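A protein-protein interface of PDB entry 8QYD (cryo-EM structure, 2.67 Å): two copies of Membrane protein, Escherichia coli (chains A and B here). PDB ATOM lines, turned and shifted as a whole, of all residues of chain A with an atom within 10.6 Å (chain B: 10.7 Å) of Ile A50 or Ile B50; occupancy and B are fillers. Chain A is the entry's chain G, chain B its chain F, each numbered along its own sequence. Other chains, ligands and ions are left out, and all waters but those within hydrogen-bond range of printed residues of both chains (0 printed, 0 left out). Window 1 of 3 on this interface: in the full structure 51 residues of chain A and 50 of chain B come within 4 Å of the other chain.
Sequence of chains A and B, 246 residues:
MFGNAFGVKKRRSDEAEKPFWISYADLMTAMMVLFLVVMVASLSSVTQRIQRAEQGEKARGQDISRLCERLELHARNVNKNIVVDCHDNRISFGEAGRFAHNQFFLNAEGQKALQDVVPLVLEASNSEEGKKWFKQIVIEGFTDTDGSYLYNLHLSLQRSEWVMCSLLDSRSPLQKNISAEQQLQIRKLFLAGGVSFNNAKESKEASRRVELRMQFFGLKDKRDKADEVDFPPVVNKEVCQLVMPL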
ATOM      1  N   SER A  42      16.962 -18.409  24.594  1.00  0.00           N
ATOM      2  CA  SER A  42      16.785 -18.182  23.166  1.00  0.00           C
ATOM      3  C   SER A  42      17.614 -17.002  22.684  1.00  0.00           C
ATOM      4  O   SER A  42      18.244 -17.074  21.622  1.00  0.00           O
ATOM      5  CB  SER A  42      15.306 -17.965  22.860  1.00  0.00           C
ATOM      6  OG  SER A  42      14.518 -18.988  23.436  1.00  0.00           O
ATOM      7  N   LEU A  43      17.625 -15.905  23.444  1.00  0.00           N
ATOM      8  CA  LEU A  43      18.412 -14.744  23.049  1.00  0.00           C
ATOM      9  C   LEU A  43      19.902 -15.040  23.111  1.00  0.00           C
ATOM     10  O   LEU A  43      20.661 -14.599  22.242  1.00  0.00           O
ATOM     11  CB  LEU A  43      18.061 -13.547  23.928  1.00  0.00           C
ATOM     12  CG  LEU A  43      16.688 -12.931  23.670  1.00  0.00           C
ATOM     13  CD1 LEU A  43      16.456 -11.742  24.578  1.00  0.00           C
ATOM     14  CD2 LEU A  43      16.556 -12.531  22.217  1.00  0.00           C
ATOM     15  N   SER A  44      20.344 -15.783  24.126  1.00  0.00           N
ATOM     16  CA  SER A  44      21.746 -16.162  24.203  1.00  0.00           C
ATOM     17  C   SER A  44      22.134 -17.154  23.118  1.00  0.00           C
ATOM     18  O   SER A  44      23.319 -17.255  22.784  1.00  0.00           O
ATOM     19  CB  SER A  44      22.055 -16.746  25.580  1.00  0.00           C
ATOM     20  OG  SER A  44      21.670 -15.847  26.603  1.00  0.00           O
ATOM     21  N   SER A  45      21.170 -17.891  22.568  1.00  0.00           N
ATOM     22  CA  SER A  45      21.481 -18.845  21.512  1.00  0.00           C
ATOM     23  C   SER A  45      21.525 -18.178  20.142  1.00  0.00           C
ATOM     24  O   SER A  45      22.417 -18.467  19.339  1.00  0.00           O
ATOM     25  CB  SER A  45      20.463 -19.984  21.523  1.00  0.00           C
ATOM     26  OG  SER A  45      20.388 -20.577  22.807  1.00  0.00           O
ATOM     27  N   VAL A  46      20.572 -17.291  19.851  1.00  0.00           N
ATOM     28  CA  VAL A  46      20.540 -16.674  18.526  1.00  0.00           C
ATOM     29  C   VAL A  46      21.750 -15.772  18.321  1.00  0.00           C
ATOM     30  O   VAL A  46      22.274 -15.659  17.206  1.00  0.00           O
ATOM     31  CB  VAL A  46      19.224 -15.907  18.299  1.00  0.00           C
ATOM     32  CG1 VAL A  46      18.074 -16.869  18.107  1.00  0.00           C
ATOM     33  CG2 VAL A  46      18.949 -14.953  19.434  1.00  0.00           C
ATOM     34  N   THR A  47      22.212 -15.112  19.380  1.00  0.00           N
ATOM     35  CA  THR A  47      23.295 -14.147  19.274  1.00  0.00           C
ATOM     36  C   THR A  47      24.642 -14.715  19.701  1.00  0.00           C
ATOM     37  O   THR A  47      25.594 -13.949  19.876  1.00  0.00           O
ATOM     38  CB  THR A  47      22.981 -12.898  20.097  1.00  0.00           C
ATOM     39  OG1 THR A  47      23.206 -13.172  21.485  1.00  0.00           O
ATOM     40  CG2 THR A  47      21.543 -12.471  19.898  1.00  0.00           C
ATOM     41  N   GLN A  48      24.753 -16.036  19.866  1.00  0.00           N
ATOM     42  CA  GLN A  48      26.009 -16.588  20.364  1.00  0.00           C
ATOM     43  C   GLN A  48      27.136 -16.406  19.357  1.00  0.00           C
ATOM     44  O   GLN A  48      28.291 -16.214  19.746  1.00  0.00           O
ATOM     45  CB  GLN A  48      25.852 -18.062  20.737  1.00  0.00           C
ATOM     46  CG  GLN A  48      25.551 -19.001  19.593  1.00  0.00           C
ATOM     47  CD  GLN A  48      25.362 -20.424  20.072  1.00  0.00           C
ATOM     48  OE1 GLN A  48      25.507 -20.713  21.258  1.00  0.00           O
ATOM     49  NE2 GLN A  48      25.045 -21.324  19.151  1.00  0.00           N
ATOM     50  N   ARG A  49      26.829 -16.471  18.060  1.00  0.00           N
ATOM     51  CA  ARG A  49      27.840 -16.134  17.063  1.00  0.00           C
ATOM     52  C   ARG A  49      28.230 -14.667  17.162  1.00  0.00           C
ATOM     53  O   ARG A  49      29.414 -14.323  17.077  1.00  0.00           O
ATOM     54  CB  ARG A  49      27.334 -16.458  15.661  1.00  0.00           C
ATOM     55  CG  ARG A  49      27.207 -17.940  15.378  1.00  0.00           C
ATOM     56  CD  ARG A  49      26.903 -18.190  13.915  1.00  0.00           C
ATOM     57  NE  ARG A  49      26.433 -19.549  13.682  1.00  0.00           N
ATOM     58  CZ  ARG A  49      25.228 -19.854  13.223  1.00  0.00           C
ATOM     59  NH1 ARG A  49      24.346 -18.916  12.926  1.00  0.00           N
ATOM     60  NH2 ARG A  49      24.900 -21.131  13.057  1.00  0.00           N
ATOM     61  N   ILE A  50      27.245 -13.790  17.357  1.00  0.00           N
ATOM     62  CA  ILE A  50      27.528 -12.369  17.522  1.00  0.00           C
ATOM     63  C   ILE A  50      28.299 -12.128  18.812  1.00  0.00           C
ATOM     64  O   ILE A  50      29.225 -11.311  18.854  1.00  0.00           O
ATOM     65  CB  ILE A  50      26.217 -11.566  17.475  1.00  0.00           C
ATOM     66  CG1 ILE A  50      25.446 -11.917  16.204  1.00  0.00           C
ATOM     67  CG2 ILE A  50      26.497 -10.078  17.535  1.00  0.00           C
ATOM     68  CD1 ILE A  50      24.179 -11.138  16.021  1.00  0.00           C
ATOM     69  N   GLN A  51      27.938 -12.840  19.883  1.00  0.00           N
ATOM     70  CA  GLN A  51      28.674 -12.713  21.138  1.00  0.00           C
ATOM     71  C   GLN A  51      30.121 -13.154  20.974  1.00  0.00           C
ATOM     72  O   GLN A  51      31.039 -12.503  21.481  1.00  0.00           O
ATOM     73  CB  GLN A  51      27.994 -13.525  22.242  1.00  0.00           C
ATOM     74  CG  GLN A  51      26.638 -13.009  22.671  1.00  0.00           C
ATOM     75  CD  GLN A  51      26.014 -13.866  23.751  1.00  0.00           C
ATOM     76  OE1 GLN A  51      26.568 -14.892  24.140  1.00  0.00           O
ATOM     77  NE2 GLN A  51      24.853 -13.450  24.243  1.00  0.00           N
ATOM     78  N   ARG A  52      30.345 -14.268  20.275  1.00  0.00           N
ATOM     79  CA  ARG A  52      31.705 -14.756  20.073  1.00  0.00           C
ATOM     80  C   ARG A  52      32.513 -13.801  19.204  1.00  0.00           C
ATOM     81  O   ARG A  52      33.691 -13.549  19.479  1.00  0.00           O
ATOM     82  CB  ARG A  52      31.675 -16.152  19.457  1.00  0.00           C
ATOM     83  CG  ARG A  52      32.999 -16.884  19.532  1.00  0.00           C
ATOM     84  CD  ARG A  52      32.897 -18.276  18.933  1.00  0.00           C
ATOM     85  NE  ARG A  52      31.643 -18.934  19.277  1.00  0.00           N
ATOM     86  CZ  ARG A  52      30.784 -19.419  18.391  1.00  0.00           C
ATOM     87  NH1 ARG A  52      31.011 -19.333  17.090  1.00  0.00           N
ATOM     88  NH2 ARG A  52      29.673 -20.010  18.819  1.00  0.00           N
ATOM     89  N   ALA A  53      31.898 -13.258  18.149  1.00  0.00           N
ATOM     90  CA  ALA A  53      32.594 -12.287  17.312  1.00  0.00           C
ATOM     91  C   ALA A  53      32.940 -11.027  18.095  1.00  0.00           C
ATOM     92  O   ALA A  53      34.035 -10.477  17.945  1.00  0.00           O
ATOM     93  CB  ALA A  53      31.745 -11.945  16.089  1.00  0.00           C
ATOM     94  N   GLU A  54      32.018 -10.556  18.937  1.00  0.00           N
ATOM     95  CA  GLU A  54      32.290  -9.370  19.743  1.00  0.00           C
ATOM     96  C   GLU A  54      33.377  -9.642  20.775  1.00  0.00           C
ATOM     97  O   GLU A  54      34.217  -8.776  21.042  1.00  0.00           O
ATOM     98  CB  GLU A  54      31.002  -8.894  20.413  1.00  0.00           C
ATOM     99  CG  GLU A  54      31.144  -7.615  21.216  1.00  0.00           C
ATOM    100  CD  GLU A  54      29.829  -7.158  21.817  1.00  0.00           C
ATOM    101  OE1 GLU A  54      28.812  -7.856  21.620  1.00  0.00           O
ATOM    102  OE2 GLU A  54      29.810  -6.101  22.482  1.00  0.00           O
ATOM    103  N   GLN A  55      33.380 -10.839  21.366  1.00  0.00           N
ATOM    104  CA  GLN A  55      34.446 -11.206  22.292  1.00  0.00           C
ATOM    105  C   GLN A  55      35.794 -11.249  21.589  1.00  0.00           C
ATOM    106  O   GLN A  55      36.801 -10.783  22.132  1.00  0.00           O
ATOM    107  CB  GLN A  55      34.144 -12.556  22.940  1.00  0.00           C
ATOM    108  CG  GLN A  55      35.220 -13.016  23.908  1.00  0.00           C
ATOM    109  CD  GLN A  55      35.362 -14.522  23.957  1.00  0.00           C
ATOM    110  OE1 GLN A  55      34.704 -15.245  23.210  1.00  0.00           O
ATOM    111  NE2 GLN A  55      36.228 -15.005  24.839  1.00  0.00           N
ATOM    112  N   GLY A  56      35.835 -11.815  20.381  1.00  0.00           N
ATOM    113  CA  GLY A  56      37.075 -11.823  19.623  1.00  0.00           C
ATOM    114  C   GLY A  56      37.541 -10.427  19.258  1.00  0.00           C
ATOM    115  O   GLY A  56      38.737 -10.133  19.293  1.00  0.00           O
ATOM    116  N   GLU A  57      36.603  -9.550  18.895  1.00  0.00           N
ATOM    117  CA  GLU A  57      36.952  -8.166  18.596  1.00  0.00           C
ATOM    118  C   GLU A  57      37.519  -7.465  19.824  1.00  0.00           C
ATOM    119  O   GLU A  57      38.511  -6.733  19.731  1.00  0.00           O
ATOM    120  CB  GLU A  57      35.725  -7.424  18.070  1.00  0.00           C
ATOM    121  CG  GLU A  57      35.924  -5.933  17.870  1.00  0.00           C
ATOM    122  CD  GLU A  57      37.107  -5.619  16.978  1.00  0.00           C
ATOM    123  OE1 GLU A  57      37.186  -6.193  15.870  1.00  0.00           O
ATOM    124  OE2 GLU A  57      37.953  -4.792  17.379  1.00  0.00           O
ATOM    125  N   LYS A  58      36.902  -7.685  20.986  1.00  0.00           N
ATOM    126  CA  LYS A  58      37.412  -7.097  22.220  1.00  0.00           C
ATOM    127  C   LYS A  58      38.792  -7.643  22.564  1.00  0.00           C
ATOM    128  O   LYS A  58      39.665  -6.896  23.017  1.00  0.00           O
ATOM    129  CB  LYS A  58      36.425  -7.353  23.360  1.00  0.00           C
ATOM    130  CG  LYS A  58      36.886  -6.864  24.719  1.00  0.00           C
ATOM    131  CD  LYS A  58      35.734  -6.851  25.712  1.00  0.00           C
ATOM    132  CE  LYS A  58      35.064  -8.212  25.808  1.00  0.00           C
ATOM    133  NZ  LYS A  58      33.604  -8.095  26.079  1.00  0.00           N
ATOM    134  N   LEU A 219      39.945  -9.950  12.069  1.00  0.00           N
ATOM    135  CA  LEU A 219      39.616 -11.149  12.834  1.00  0.00           C
ATOM    136  C   LEU A 219      39.611 -12.388  11.948  1.00  0.00           C
ATOM    137  O   LEU A 219      40.087 -13.454  12.356  1.00  0.00           O
ATOM    138  CB  LEU A 219      38.268 -10.982  13.531  1.00  0.00           C
ATOM    139  CG  LEU A 219      38.251 -10.089  14.771  1.00  0.00           C
ATOM    140  CD1 LEU A 219      36.888  -9.446  14.949  1.00  0.00           C
ATOM    141  CD2 LEU A 219      38.628 -10.895  15.999  1.00  0.00           C
ATOM    142  N   LYS A 220      39.078 -12.271  10.735  1.00  0.00           N
ATOM    143  CA  LYS A 220      38.947 -13.412   9.839  1.00  0.00           C
ATOM    144  C   LYS A 220      40.131 -13.573   8.894  1.00  0.00           C
ATOM    145  O   LYS A 220      40.146 -14.520   8.101  1.00  0.00           O
ATOM    146  CB  LYS A 220      37.652 -13.297   9.028  1.00  0.00           C
ATOM    147  CG  LYS A 220      36.379 -13.324   9.868  1.00  0.00           C
ATOM    148  CD  LYS A 220      36.519 -14.232  11.082  1.00  0.00           C
ATOM    149  CE  LYS A 220      35.183 -14.439  11.774  1.00  0.00           C
ATOM    150  NZ  LYS A 220      35.242 -15.537  12.778  1.00  0.00           N
ATOM    151  N   SER B  42      10.867  -9.954  21.749  1.00  0.00           N
ATOM    152  CA  SER B  42      12.314  -9.800  21.747  1.00  0.00           C
ATOM    153  C   SER B  42      12.976 -10.803  20.816  1.00  0.00           C
ATOM    154  O   SER B  42      13.914 -10.455  20.093  1.00  0.00           O
ATOM    155  CB  SER B  42      12.855  -9.948  23.167  1.00  0.00           C
ATOM    156  OG  SER B  42      12.644  -8.766  23.914  1.00  0.00           O
ATOM    157  N   LEU B  43      12.507 -12.053  20.816  1.00  0.00           N
ATOM    158  CA  LEU B  43      13.075 -13.041  19.908  1.00  0.00           C
ATOM    159  C   LEU B  43      12.856 -12.634  18.458  1.00  0.00           C
ATOM    160  O   LEU B  43      13.789 -12.662  17.643  1.00  0.00           O
ATOM    161  CB  LEU B  43      12.469 -14.413  20.186  1.00  0.00           C
ATOM    162  CG  LEU B  43      13.314 -15.599  19.726  1.00  0.00           C
ATOM    163  CD1 LEU B  43      14.735 -15.468  20.246  1.00  0.00           C
ATOM    164  CD2 LEU B  43      12.689 -16.903  20.180  1.00  0.00           C
ATOM    165  N   SER B  44      11.630 -12.226  18.124  1.00  0.00           N
ATOM    166  CA  SER B  44      11.337 -11.787  16.766  1.00  0.00           C
ATOM    167  C   SER B  44      12.179 -10.580  16.383  1.00  0.00           C
ATOM    168  O   SER B  44      12.744 -10.534  15.287  1.00  0.00           O
ATOM    169  CB  SER B  44       9.849 -11.467  16.634  1.00  0.00           C
ATOM    170  OG  SER B  44       9.533 -11.019  15.330  1.00  0.00           O
ATOM    171  N   SER B  45      12.296  -9.601  17.283  1.00  0.00           N
ATOM    172  CA  SER B  45      13.054  -8.393  16.981  1.00  0.00           C
ATOM    173  C   SER B  45      14.531  -8.693  16.769  1.00  0.00           C
ATOM    174  O   SER B  45      15.141  -8.189  15.822  1.00  0.00           O
ATOM    175  CB  SER B  45      12.869  -7.375  18.106  1.00  0.00           C
ATOM    176  OG  SER B  45      13.698  -6.246  17.916  1.00  0.00           O
ATOM    177  N   VAL B  46      15.129  -9.506  17.641  1.00  0.00           N
ATOM    178  CA  VAL B  46      16.549  -9.809  17.506  1.00  0.00           C
ATOM    179  C   VAL B  46      16.808 -10.596  16.229  1.00  0.00           C
ATOM    180  O   VAL B  46      17.777 -10.327  15.505  1.00  0.00           O
ATOM    181  CB  VAL B  46      17.058 -10.554  18.751  1.00  0.00           C
ATOM    182  CG1 VAL B  46      18.464 -11.065  18.521  1.00  0.00           C
ATOM    183  CG2 VAL B  46      17.026  -9.635  19.956  1.00  0.00           C
ATOM    184  N   THR B  47      15.949 -11.571  15.924  1.00  0.00           N
ATOM    185  CA  THR B  47      16.101 -12.307  14.676  1.00  0.00           C
ATOM    186  C   THR B  47      15.962 -11.382  13.474  1.00  0.00           C
ATOM    187  O   THR B  47      16.672 -11.539  12.475  1.00  0.00           O
ATOM    188  CB  THR B  47      15.079 -13.440  14.617  1.00  0.00           C
ATOM    189  OG1 THR B  47      15.293 -14.326  15.720  1.00  0.00           O
ATOM    190  CG2 THR B  47      15.214 -14.219  13.320  1.00  0.00           C
ATOM    191  N   GLN B  48      15.055 -10.404  13.555  1.00  0.00           N
ATOM    192  CA  GLN B  48      14.881  -9.471  12.449  1.00  0.00           C
ATOM    193  C   GLN B  48      16.104  -8.579  12.271  1.00  0.00           C
ATOM    194  O   GLN B  48      16.514  -8.317  11.140  1.00  0.00           O
ATOM    195  CB  GLN B  48      13.622  -8.632  12.653  1.00  0.00           C
ATOM    196  CG  GLN B  48      12.330  -9.401  12.438  1.00  0.00           C
ATOM    197  CD  GLN B  48      11.111  -8.504  12.422  1.00  0.00           C
ATOM    198  OE1 GLN B  48      11.081  -7.493  11.725  1.00  0.00           O
ATOM    199  NE2 GLN B  48      10.099  -8.868  13.198  1.00  0.00           N
ATOM    200  N   ARG B  49      16.700  -8.100  13.368  1.00  0.00           N
ATOM    201  CA  ARG B  49      17.965  -7.371  13.249  1.00  0.00           C
ATOM    202  C   ARG B  49      19.050  -8.228  12.609  1.00  0.00           C
ATOM    203  O   ARG B  49      19.795  -7.756  11.741  1.00  0.00           O
ATOM    204  CB  ARG B  49      18.450  -6.850  14.604  1.00  0.00           C
ATOM    205  CG  ARG B  49      17.889  -5.511  15.054  1.00  0.00           C
ATOM    206  CD  ARG B  49      16.480  -5.547  15.537  1.00  0.00           C
ATOM    207  NE  ARG B  49      16.058  -4.236  16.012  1.00  0.00           N
ATOM    208  CZ  ARG B  49      16.219  -3.804  17.253  1.00  0.00           C
ATOM    209  NH1 ARG B  49      16.790  -4.557  18.177  1.00  0.00           N
ATOM    210  NH2 ARG B  49      15.796  -2.585  17.574  1.00  0.00           N
ATOM    211  N   ILE B  50      19.171  -9.486  13.037  1.00  0.00           N
ATOM    212  CA  ILE B  50      20.230 -10.339  12.501  1.00  0.00           C
ATOM    213  C   ILE B  50      20.038 -10.557  11.004  1.00  0.00           C
ATOM    214  O   ILE B  50      20.975 -10.402  10.208  1.00  0.00           O
ATOM    215  CB  ILE B  50      20.287 -11.671  13.268  1.00  0.00           C
ATOM    216  CG1 ILE B  50      20.644 -11.427  14.733  1.00  0.00           C
ATOM    217  CG2 ILE B  50      21.290 -12.611  12.630  1.00  0.00           C
ATOM    218  CD1 ILE B  50      20.471 -12.638  15.607  1.00  0.00           C
ATOM    219  N   GLN B  51      18.813 -10.898  10.593  1.00  0.00           N
ATOM    220  CA  GLN B  51      18.577 -11.138   9.174  1.00  0.00           C
ATOM    221  C   GLN B  51      18.664  -9.848   8.369  1.00  0.00           C
ATOM    222  O   GLN B  51      19.107  -9.874   7.220  1.00  0.00           O
ATOM    223  CB  GLN B  51      17.229 -11.827   8.954  1.00  0.00           C
ATOM    224  CG  GLN B  51      16.012 -11.005   9.321  1.00  0.00           C
ATOM    225  CD  GLN B  51      14.717 -11.773   9.131  1.00  0.00           C
ATOM    226  OE1 GLN B  51      14.723 -12.916   8.676  1.00  0.00           O
ATOM    227  NE2 GLN B  51      13.599 -11.142   9.471  1.00  0.00           N
ATOM    228  N   ARG B  52      18.270  -8.714   8.951  1.00  0.00           N
ATOM    229  CA  ARG B  52      18.423  -7.436   8.268  1.00  0.00           C
ATOM    230  C   ARG B  52      19.885  -7.120   8.009  1.00  0.00           C
ATOM    231  O   ARG B  52      20.243  -6.684   6.910  1.00  0.00           O
ATOM    232  CB  ARG B  52      17.780  -6.325   9.093  1.00  0.00           C
ATOM    233  CG  ARG B  52      17.848  -4.960   8.447  1.00  0.00           C
ATOM    234  CD  ARG B  52      17.122  -3.933   9.289  1.00  0.00           C
ATOM    235  NE  ARG B  52      15.684  -4.162   9.300  1.00  0.00           N
ATOM    236  CZ  ARG B  52      14.831  -3.521  10.087  1.00  0.00           C
ATOM    237  NH1 ARG B  52      15.245  -2.632  10.973  1.00  0.00           N
ATOM    238  NH2 ARG B  52      13.532  -3.781   9.982  1.00  0.00           N
ATOM    239  N   ALA B  53      20.746  -7.328   9.005  1.00  0.00           N
ATOM    240  CA  ALA B  53      22.170  -7.095   8.799  1.00  0.00           C
ATOM    241  C   ALA B  53      22.730  -8.037   7.742  1.00  0.00           C
ATOM    242  O   ALA B  53      23.512  -7.620   6.875  1.00  0.00           O
ATOM    243  CB  ALA B  53      22.926  -7.252  10.117  1.00  0.00           C
ATOM    244  N   GLU B  54      22.331  -9.312   7.788  1.00  0.00           N
ATOM    245  CA  GLU B  54      22.830 -10.272   6.808  1.00  0.00           C
ATOM    246  C   GLU B  54      22.415  -9.886   5.393  1.00  0.00           C
ATOM    247  O   GLU B  54      23.237  -9.894   4.468  1.00  0.00           O
ATOM    248  CB  GLU B  54      22.336 -11.677   7.154  1.00  0.00           C
ATOM    249  CG  GLU B  54      23.061 -12.311   8.328  1.00  0.00           C
ATOM    250  CD  GLU B  54      22.372 -13.565   8.832  1.00  0.00           C
ATOM    251  OE1 GLU B  54      21.249 -13.857   8.373  1.00  0.00           O
ATOM    252  OE2 GLU B  54      22.957 -14.262   9.688  1.00  0.00           O
ATOM    253  N   GLN B  55      21.144  -9.521   5.205  1.00  0.00           N
ATOM    254  CA  GLN B  55      20.680  -9.178   3.865  1.00  0.00           C
ATOM    255  C   GLN B  55      21.226  -7.836   3.403  1.00  0.00           C
ATOM    256  O   GLN B  55      21.438  -7.646   2.205  1.00  0.00           O
ATOM    257  CB  GLN B  55      19.153  -9.189   3.798  1.00  0.00           C
ATOM    258  CG  GLN B  55      18.509 -10.461   4.333  1.00  0.00           C
ATOM    259  CD  GLN B  55      18.581 -11.629   3.363  1.00  0.00           C
ATOM    260  OE1 GLN B  55      19.317 -11.597   2.377  1.00  0.00           O
ATOM    261  NE2 GLN B  55      17.811 -12.674   3.645  1.00  0.00           N
ATOM    262  N   GLY B  56      21.473  -6.898   4.319  1.00  0.00           N
ATOM    263  CA  GLY B  56      22.128  -5.663   3.926  1.00  0.00           C
ATOM    264  C   GLY B  56      23.550  -5.892   3.452  1.00  0.00           C
ATOM    265  O   GLY B  56      23.982  -5.318   2.446  1.00  0.00           O
ATOM    266  N   GLU B  57      24.295  -6.745   4.162  1.00  0.00           N
ATOM    267  CA  GLU B  57      25.638  -7.095   3.714  1.00  0.00           C
ATOM    268  C   GLU B  57      25.598  -7.805   2.366  1.00  0.00           C
ATOM    269  O   GLU B  57      26.424  -7.533   1.483  1.00  0.00           O
ATOM    270  CB  GLU B  57      26.326  -7.969   4.761  1.00  0.00           C
ATOM    271  CG  GLU B  57      27.828  -8.058   4.595  1.00  0.00           C
ATOM    272  CD  GLU B  57      28.504  -6.709   4.722  1.00  0.00           C
ATOM    273  OE1 GLU B  57      28.520  -6.155   5.841  1.00  0.00           O
ATOM    274  OE2 GLU B  57      29.017  -6.202   3.703  1.00  0.00           O
ATOM    275  N   LYS B  58      24.636  -8.712   2.184  1.00  0.00           N
ATOM    276  CA  LYS B  58      24.511  -9.406   0.906  1.00  0.00           C
ATOM    277  C   LYS B  58      24.160  -8.439  -0.219  1.00  0.00           C
ATOM    278  O   LYS B  58      24.666  -8.575  -1.335  1.00  0.00           O
ATOM    279  CB  LYS B  58      23.465 -10.513   1.006  1.00  0.00           C
ATOM    280  CG  LYS B  58      23.615 -11.589  -0.053  1.00  0.00           C
ATOM    281  CD  LYS B  58      22.494 -12.611   0.026  1.00  0.00           C
ATOM    282  CE  LYS B  58      21.183 -12.029  -0.473  1.00  0.00           C
ATOM    283  NZ  LYS B  58      20.129 -13.073  -0.601  1.00  0.00           N
ATOM    284  N   LEU B 219      29.859  -1.651   5.323  1.00  0.00           N
ATOM    285  CA  LEU B 219      28.466  -1.493   5.727  1.00  0.00           C
ATOM    286  C   LEU B 219      28.334  -0.490   6.867  1.00  0.00           C
ATOM    287  O   LEU B 219      27.382   0.298   6.903  1.00  0.00           O
ATOM    288  CB  LEU B 219      27.880  -2.846   6.125  1.00  0.00           C
ATOM    289  CG  LEU B 219      26.358  -2.954   6.084  1.00  0.00           C
ATOM    290  CD1 LEU B 219      25.853  -2.805   4.660  1.00  0.00           C
ATOM    291  CD2 LEU B 219      25.904  -4.276   6.676  1.00  0.00           C
ATOM    292  N   LYS B 220      29.279  -0.505   7.807  1.00  0.00           N
ATOM    293  CA  LYS B 220      29.239   0.405   8.944  1.00  0.00           C
ATOM    294  C   LYS B 220      29.945   1.728   8.674  1.00  0.00           C
ATOM    295  O   LYS B 220      29.871   2.630   9.516  1.00  0.00           O
ATOM    296  CB  LYS B 220      29.863  -0.264  10.169  1.00  0.00           C
ATOM    297  CG  LYS B 220      29.169  -1.546  10.592  1.00  0.00           C
ATOM    298  CD  LYS B 220      27.755  -1.283  11.070  1.00  0.00           C
ATOM    299  CE  LYS B 220      27.134  -2.545  11.644  1.00  0.00           C
ATOM    300  NZ  LYS B 220      26.877  -3.563  10.586  1.00  0.00           N
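O of Leu B43 is in hydrogen-bond range of OG1 of Thr B47, 3.0 Å away. O of Leu A43 lies within hydrogen-bond range of OG1 of Thr A47 (3.0 Å). OG1 of Thr A47 is in hydrogen-bond range of NE2 of Gln A51 (3.2 Å).
Printed residues of chain B that touch a printed residue of chain A: Ser B42, Leu B43, Val B46 and Ile B50. Hydrophobic or aromatic side chains of chain B that line the printed part of chain A: Leu B43, Val B46 and Ile B50. Of the 19 printed residues of chain A, 5 touch a printed residue of chain B. Hydrophobic or aromatic side chains of chain A that line the printed part of chain B: Leu A43 and Ile A50. Among the printed residues, no Asp or Glu carboxylate lies within 4 Å of a Lys or Arg side-chain nitrogen of the other chain.
Among the printed residues, merely in contact across the chains: Ser A42 with Leu B43 (3.7 Å), Leu A43 with Ser B42 (3.98 Å), Leu A43 with Leu B43 (3.98 Å), Leu A43 with Val B46 (3.7 Å), Val A46 with Ile B50 (3.9 Å), Thr A47 with Val B46 (3.7 Å) and Ile A50 with Ile B50 (3.8 Å).
Of chain B, only Ile B50 comes within 4 Å of Ile A50. Ile B50 touches just these residues of chain A: Val A46 (3.9 Å) and Ile A50 (3.8 Å). Val A46 touches one residue of chain B. No residue of chain B comes within 4 Å of Ala A53. Of chain A, only Leu A43 and Thr A47 come within 4 Å of Val B46. Ala B53 touches none of the printed residues of chain A. No residue of chain A comes within 4 Å of Glu B54. Of the printed residues of chain B, Ser A42 touches Leu B43 (3.7 Å). Printed residues of chain B within 4 Å of Leu A43: Ser B42 (3.98 Å), Leu B43 (3.98 Å) and Val B46 (3.7 Å). Printed residues of chain A within 4 Å of Ser B42: Leu A43. Of the printed residues of chain A, Leu B43 touches Ser A42 (3.7 Å) and Leu A43 (3.98 Å). The nearest residue of chain B that does not touch Ile A50 is Val B46 (6.2 Å). The nearest residue of chain A that does not touch Ile B50 is Thr A47 (4.4 Å). The nearest printed residue of chain A that does not touch Leu B43 is Val A46 (4.2 Å).
Ser A42 touches Leu B43, and with the chains exchanged Leu A43 touches Ser B42. Leu A43 touches its own counterpart, Leu B43. Leu A43 touches Val B46, but with the chains exchanged Val A46 does not touch Leu B43 (4.2 Å). Ile A50 touches its own counterpart, Ile B50. Positions printed for both chains: 42, 43, 44, 45, 46, 47, 48, 49, 50, 51, 52, 53, 54, 55, 56, 57, 58, 219 and 220. Of the 7 pairs that touch across the chains among the printed residues, 4 have their exchanged pair printed and touching as well.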
